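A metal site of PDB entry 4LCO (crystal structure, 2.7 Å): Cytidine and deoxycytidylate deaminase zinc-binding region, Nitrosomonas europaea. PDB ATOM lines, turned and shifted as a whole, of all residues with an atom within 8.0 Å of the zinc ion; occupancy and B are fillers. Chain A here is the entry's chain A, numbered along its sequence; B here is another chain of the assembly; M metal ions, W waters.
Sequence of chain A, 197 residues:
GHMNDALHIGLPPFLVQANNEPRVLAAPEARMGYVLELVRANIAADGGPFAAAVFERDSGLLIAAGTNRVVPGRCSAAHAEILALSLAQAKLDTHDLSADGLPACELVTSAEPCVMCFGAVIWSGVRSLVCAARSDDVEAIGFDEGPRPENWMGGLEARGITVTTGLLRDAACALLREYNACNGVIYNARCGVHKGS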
ATOM      1  N   PHE A  50      27.542   5.876  15.915  1.00  0.00           N
ATOM      2  CA  PHE A  50      27.550   6.715  17.109  1.00  0.00           C
ATOM      3  C   PHE A  50      28.932   7.260  17.406  1.00  0.00           C
ATOM      4  O   PHE A  50      29.949   6.542  17.334  1.00  0.00           O
ATOM      5  CB  PHE A  50      27.022   5.948  18.307  1.00  0.00           C
ATOM      6  CG  PHE A  50      25.612   5.425  18.142  1.00  0.00           C
ATOM      7  CD1 PHE A  50      24.504   6.239  18.445  1.00  0.00           C
ATOM      8  CD2 PHE A  50      25.370   4.133  17.689  1.00  0.00           C
ATOM      9  CE1 PHE A  50      23.188   5.752  18.307  1.00  0.00           C
ATOM     10  CE2 PHE A  50      24.066   3.641  17.545  1.00  0.00           C
ATOM     11  CZ  PHE A  50      22.970   4.450  17.842  1.00  0.00           C
ATOM     12  N   ASN A  68      31.430   4.303  18.808  1.00  0.00           N
ATOM     13  CA  ASN A  68      31.143   2.884  19.064  1.00  0.00           C
ATOM     14  C   ASN A  68      32.203   1.916  18.533  1.00  0.00           C
ATOM     15  O   ASN A  68      32.415   1.800  17.320  1.00  0.00           O
ATOM     16  CB  ASN A  68      29.809   2.534  18.471  1.00  0.00           C
ATOM     17  CG  ASN A  68      28.714   2.385  19.512  1.00  0.00           C
ATOM     18  OD1 ASN A  68      28.427   3.309  20.327  1.00  0.00           O
ATOM     19  ND2 ASN A  68      28.081   1.213  19.496  1.00  0.00           N
ATOM     20  N   VAL A  70      32.254  -1.280  19.692  1.00  0.00           N
ATOM     21  CA  VAL A  70      31.675  -2.462  20.355  1.00  0.00           C
ATOM     22  C   VAL A  70      32.128  -3.768  19.676  1.00  0.00           C
ATOM     23  O   VAL A  70      32.857  -4.578  20.267  1.00  0.00           O
ATOM     24  CB  VAL A  70      30.104  -2.374  20.439  1.00  0.00           C
ATOM     25  CG1 VAL A  70      29.455  -3.711  20.830  1.00  0.00           C
ATOM     26  CG2 VAL A  70      29.649  -1.251  21.364  1.00  0.00           C
ATOM     27  N   SER A  76      31.093  -4.810  24.803  1.00  0.00           N
ATOM     28  CA  SER A  76      29.760  -4.219  24.862  1.00  0.00           C
ATOM     29  C   SER A  76      29.754  -2.865  25.595  1.00  0.00           C
ATOM     30  O   SER A  76      28.784  -2.102  25.540  1.00  0.00           O
ATOM     31  CB  SER A  76      28.760  -5.205  25.482  1.00  0.00           C
ATOM     32  OG  SER A  76      29.269  -5.799  26.659  1.00  0.00           O
ATOM     33  N   ALA A  77      30.861  -2.560  26.258  1.00  0.00           N
ATOM     34  CA  ALA A  77      30.919  -1.369  27.065  1.00  0.00           C
ATOM     35  C   ALA A  77      31.508  -0.219  26.293  1.00  0.00           C
ATOM     36  O   ALA A  77      31.516   0.919  26.768  1.00  0.00           O
ATOM     37  CB  ALA A  77      31.713  -1.605  28.330  1.00  0.00           C
ATOM     38  N   ALA A  78      31.986  -0.511  25.085  1.00  0.00           N
ATOM     39  CA  ALA A  78      32.759   0.459  24.322  1.00  0.00           C
ATOM     40  C   ALA A  78      31.906   1.415  23.464  1.00  0.00           C
ATOM     41  O   ALA A  78      32.217   1.648  22.290  1.00  0.00           O
ATOM     42  CB  ALA A  78      33.807  -0.252  23.489  1.00  0.00           C
ATOM     43  N   HIS A  79      30.825   1.927  24.050  1.00  0.00           N
ATOM     44  CA  HIS A  79      30.091   3.047  23.470  1.00  0.00           C
ATOM     45  C   HIS A  79      30.926   4.303  23.337  1.00  0.00           C
ATOM     46  O   HIS A  79      31.849   4.564  24.086  1.00  0.00           O
ATOM     47  CB  HIS A  79      28.869   3.353  24.329  1.00  0.00           C
ATOM     48  CG  HIS A  79      27.789   2.298  24.260  1.00  0.00           C
ATOM     49  ND1 HIS A  79      26.571   2.451  24.857  1.00  0.00           N
ATOM     50  CD2 HIS A  79      27.770   1.058  23.657  1.00  0.00           C
ATOM     51  CE1 HIS A  79      25.823   1.369  24.635  1.00  0.00           C
ATOM     52  NE2 HIS A  79      26.551   0.512  23.899  1.00  0.00           N
ATOM     53  N   ALA A  80      30.567   5.092  22.342  1.00  0.00           N
ATOM     54  CA  ALA A  80      31.163   6.403  22.067  1.00  0.00           C
ATOM     55  C   ALA A  80      31.305   7.248  23.308  1.00  0.00           C
ATOM     56  O   ALA A  80      32.376   7.815  23.567  1.00  0.00           O
ATOM     57  CB  ALA A  80      30.306   7.137  21.038  1.00  0.00           C
ATOM     58  N   GLU A  81      30.229   7.325  24.104  1.00  0.00           N
ATOM     59  CA  GLU A  81      30.228   8.156  25.270  1.00  0.00           C
ATOM     60  C   GLU A  81      31.329   7.737  26.234  1.00  0.00           C
ATOM     61  O   GLU A  81      32.054   8.573  26.763  1.00  0.00           O
ATOM     62  CB  GLU A  81      28.859   8.125  25.949  1.00  0.00           C
ATOM     63  CG  GLU A  81      27.698   8.571  25.078  1.00  0.00           C
ATOM     64  CD  GLU A  81      27.093   7.386  24.362  1.00  0.00           C
ATOM     65  OE1 GLU A  81      27.897   6.688  23.703  1.00  0.00           O
ATOM     66  OE2 GLU A  81      25.858   7.117  24.498  1.00  0.00           O
ATOM     67  N   ILE A  82      31.438   6.423  26.446  1.00  0.00           N
ATOM     68  CA  ILE A  82      32.363   5.832  27.396  1.00  0.00           C
ATOM     69  C   ILE A  82      33.796   6.098  26.982  1.00  0.00           C
ATOM     70  O   ILE A  82      34.646   6.392  27.829  1.00  0.00           O
ATOM     71  CB  ILE A  82      32.072   4.320  27.517  1.00  0.00           C
ATOM     72  CG1 ILE A  82      30.651   4.118  27.972  1.00  0.00           C
ATOM     73  CG2 ILE A  82      32.982   3.614  28.529  1.00  0.00           C
ATOM     74  CD1 ILE A  82      30.347   4.689  29.327  1.00  0.00           C
ATOM     75  N   THR A 109      27.147  14.405  22.024  1.00  0.00           N
ATOM     76  CA  THR A 109      26.804  13.095  21.448  1.00  0.00           C
ATOM     77  C   THR A 109      25.842  13.139  20.287  1.00  0.00           C
ATOM     78  O   THR A 109      24.894  13.901  20.312  1.00  0.00           O
ATOM     79  CB  THR A 109      26.178  12.134  22.452  1.00  0.00           C
ATOM     80  OG1 THR A 109      27.011  12.068  23.590  1.00  0.00           O
ATOM     81  CG2 THR A 109      26.133  10.748  21.880  1.00  0.00           C
ATOM     82  N   ALA A 111      23.756  10.939  19.608  1.00  0.00           N
ATOM     83  CA  ALA A 111      22.441  10.434  19.997  1.00  0.00           C
ATOM     84  C   ALA A 111      22.276  10.414  21.500  1.00  0.00           C
ATOM     85  O   ALA A 111      23.261  10.317  22.240  1.00  0.00           O
ATOM     86  CB  ALA A 111      22.199   9.040  19.439  1.00  0.00           C
ATOM     87  N   GLU A 112      21.029  10.521  21.939  1.00  0.00           N
ATOM     88  CA  GLU A 112      20.671  10.379  23.318  1.00  0.00           C
ATOM     89  C   GLU A 112      21.281   9.084  23.907  1.00  0.00           C
ATOM     90  O   GLU A 112      21.245   8.029  23.273  1.00  0.00           O
ATOM     91  CB  GLU A 112      19.150  10.441  23.459  1.00  0.00           C
ATOM     92  CG  GLU A 112      18.682  11.902  23.450  1.00  0.00           C
ATOM     93  CD  GLU A 112      17.183  12.124  23.471  1.00  0.00           C
ATOM     94  OE1 GLU A 112      16.434  11.267  23.986  1.00  0.00           O
ATOM     95  OE2 GLU A 112      16.750  13.193  22.985  1.00  0.00           O
ATOM     96  N   PRO A 113      21.887   9.203  25.097  1.00  0.00           N
ATOM     97  CA  PRO A 113      22.688   8.137  25.735  1.00  0.00           C
ATOM     98  C   PRO A 113      21.833   7.026  26.324  1.00  0.00           C
ATOM     99  O   PRO A 113      20.761   7.311  26.890  1.00  0.00           O
ATOM    100  CB  PRO A 113      23.386   8.884  26.858  1.00  0.00           C
ATOM    101  CG  PRO A 113      22.385   9.925  27.265  1.00  0.00           C
ATOM    102  CD  PRO A 113      21.777  10.397  25.968  1.00  0.00           C
ATOM    103  N   CYS A 114      22.293   5.782  26.173  1.00  0.00           N
ATOM    104  CA  CYS A 114      21.635   4.614  26.765  1.00  0.00           C
ATOM    105  C   CYS A 114      21.888   4.634  28.287  1.00  0.00           C
ATOM    106  O   CYS A 114      22.712   5.421  28.785  1.00  0.00           O
ATOM    107  CB  CYS A 114      22.182   3.344  26.149  1.00  0.00           C
ATOM    108  SG  CYS A 114      23.814   2.961  26.785  1.00  0.00           S
ATOM    109  N   VAL A 115      21.194   3.778  29.034  1.00  0.00           N
ATOM    110  CA  VAL A 115      21.296   3.841  30.485  1.00  0.00           C
ATOM    111  C   VAL A 115      22.727   3.753  30.984  1.00  0.00           C
ATOM    112  O   VAL A 115      23.106   4.504  31.864  1.00  0.00           O
ATOM    113  CB  VAL A 115      20.489   2.782  31.232  1.00  0.00           C
ATOM    114  CG1 VAL A 115      19.976   3.381  32.530  1.00  0.00           C
ATOM    115  CG2 VAL A 115      19.347   2.285  30.363  1.00  0.00           C
ATOM    116  N   MET A 116      23.522   2.825  30.442  1.00  0.00           N
ATOM    117  CA  MET A 116      24.903   2.694  30.875  1.00  0.00           C
ATOM    118  C   MET A 116      25.620   4.059  30.804  1.00  0.00           C
ATOM    119  O   MET A 116      26.199   4.518  31.799  1.00  0.00           O
ATOM    120  CB  MET A 116      25.601   1.635  30.035  1.00  0.00           C
ATOM    121  CG  MET A 116      27.138   1.657  30.082  1.00  0.00           C
ATOM    122  SD  MET A 116      27.940   0.490  28.964  1.00  0.00           S
ATOM    123  CE  MET A 116      27.946   1.398  27.440  1.00  0.00           C
ATOM    124  N   CYS A 117      25.528   4.730  29.646  1.00  0.00           N
ATOM    125  CA  CYS A 117      26.229   5.973  29.387  1.00  0.00           C
ATOM    126  C   CYS A 117      25.515   7.112  30.076  1.00  0.00           C
ATOM    127  O   CYS A 117      26.116   8.160  30.334  1.00  0.00           O
ATOM    128  CB  CYS A 117      26.357   6.208  27.889  1.00  0.00           C
ATOM    129  SG  CYS A 117      26.988   4.762  26.990  1.00  0.00           S
ATOM    130  N   PHE A 118      24.240   6.906  30.372  1.00  0.00           N
ATOM    131  CA  PHE A 118      23.523   7.830  31.248  1.00  0.00           C
ATOM    132  C   PHE A 118      24.178   7.935  32.651  1.00  0.00           C
ATOM    133  O   PHE A 118      24.462   9.030  33.109  1.00  0.00           O
ATOM    134  CB  PHE A 118      22.063   7.409  31.322  1.00  0.00           C
ATOM    135  CG  PHE A 118      21.333   7.989  32.485  1.00  0.00           C
ATOM    136  CD1 PHE A 118      20.958   9.323  32.481  1.00  0.00           C
ATOM    137  CD2 PHE A 118      20.975   7.181  33.568  1.00  0.00           C
ATOM    138  CE1 PHE A 118      20.256   9.850  33.553  1.00  0.00           C
ATOM    139  CE2 PHE A 118      20.272   7.708  34.640  1.00  0.00           C
ATOM    140  CZ  PHE A 118      19.907   9.045  34.636  1.00  0.00           C
ATOM    141  N   ALA A 120      27.374   6.735  33.233  1.00  0.00           N
ATOM    142  CA  ALA A 120      28.696   7.280  32.846  1.00  0.00           C
ATOM    143  C   ALA A 120      28.762   8.779  32.890  1.00  0.00           C
ATOM    144  O   ALA A 120      29.790   9.321  33.251  1.00  0.00           O
ATOM    145  CB  ALA A 120      29.105   6.839  31.444  1.00  0.00           C
ATOM    146  N   ASP A 144      18.982  -0.451  21.098  1.00  0.00           N
ATOM    147  CA  ASP A 144      18.176  -0.319  22.298  1.00  0.00           C
ATOM    148  C   ASP A 144      18.770   0.716  23.282  1.00  0.00           C
ATOM    149  O   ASP A 144      19.958   0.657  23.623  1.00  0.00           O
ATOM    150  CB  ASP A 144      17.981  -1.684  22.972  1.00  0.00           C
ATOM    151  CG  ASP A 144      16.927  -1.664  24.080  1.00  0.00           C
ATOM    152  OD1 ASP A 144      16.234  -0.643  24.244  1.00  0.00           O
ATOM    153  OD2 ASP A 144      16.780  -2.685  24.777  1.00  0.00           O
ATOM    154  N   GLU A 145      17.939   1.653  23.728  1.00  0.00           N
ATOM    155  CA  GLU A 145      18.349   2.574  24.788  1.00  0.00           C
ATOM    156  C   GLU A 145      18.457   1.926  26.166  1.00  0.00           C
ATOM    157  O   GLU A 145      19.283   2.328  26.994  1.00  0.00           O
ATOM    158  CB  GLU A 145      17.419   3.775  24.869  1.00  0.00           C
ATOM    159  CG  GLU A 145      17.562   4.760  23.733  1.00  0.00           C
ATOM    160  CD  GLU A 145      18.971   5.339  23.544  1.00  0.00           C
ATOM    161  OE1 GLU A 145      19.057   6.319  22.772  1.00  0.00           O
ATOM    162  OE2 GLU A 145      19.965   4.846  24.129  1.00  0.00           O
ATOM    163  N   TRP B 123      23.732  -5.047  28.299  1.00  0.00           N
ATOM    164  CA  TRP B 123      24.414  -5.254  26.992  1.00  0.00           C
ATOM    165  C   TRP B 123      25.447  -6.350  26.970  1.00  0.00           C
ATOM    166  O   TRP B 123      25.860  -6.760  25.894  1.00  0.00           O
ATOM    167  CB  TRP B 123      25.076  -3.965  26.479  1.00  0.00           C
ATOM    168  CG  TRP B 123      24.276  -2.709  26.678  1.00  0.00           C
ATOM    169  CD1 TRP B 123      24.714  -1.500  27.239  1.00  0.00           C
ATOM    170  CD2 TRP B 123      22.868  -2.488  26.373  1.00  0.00           C
ATOM    171  NE1 TRP B 123      23.702  -0.569  27.269  1.00  0.00           N
ATOM    172  CE2 TRP B 123      22.572  -1.093  26.771  1.00  0.00           C
ATOM    173  CE3 TRP B 123      21.870  -3.261  25.801  1.00  0.00           C
ATOM    174  CZ2 TRP B 123      21.322  -0.541  26.589  1.00  0.00           C
ATOM    175  CZ3 TRP B 123      20.595  -2.696  25.658  1.00  0.00           C
ATOM    176  CH2 TRP B 123      20.343  -1.373  26.035  1.00  0.00           C
HETATM  177 ZN    ZN M   1      25.595   3.916  25.602  1.00  0.00          ZN
HETATM  178  O   HOH W   1      24.511   4.660  24.325  1.00  0.00           O
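Residues that only touch the zinc ion: Glu 81 (3.4 Å) and Met 116 (3.9 Å).
Five residues have an atom within 4 Å of the zinc ion: His 79, Glu 81, Cys 114, Met 116 and Cys 117.
The backbone NH of Cys 114 lies close to the side-chain carboxylate of Glu 145 (3.2 Å).
The backbone NH (N) of Met 116 sits close to the side-chain sulfur (SG) of Cys 114.
SG of Cys 114 lies close to NE1 of Trp 123 of chain B, at 3.6 Å.
The side-chain carboxylate of Glu 81 sits close to the side-chain sulfur of Cys 117.
Water W1 lies within hydrogen-bond range of the side-chain carboxylate of Glu 81 and the backbone NH of Cys 114.
The zinc ion is bound by water W1 (1.8 Å), ND1 of His 79 (1.9 Å), SG of Cys 117 (2.1 Å) and SG of Cys 114 (2.3 Å).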
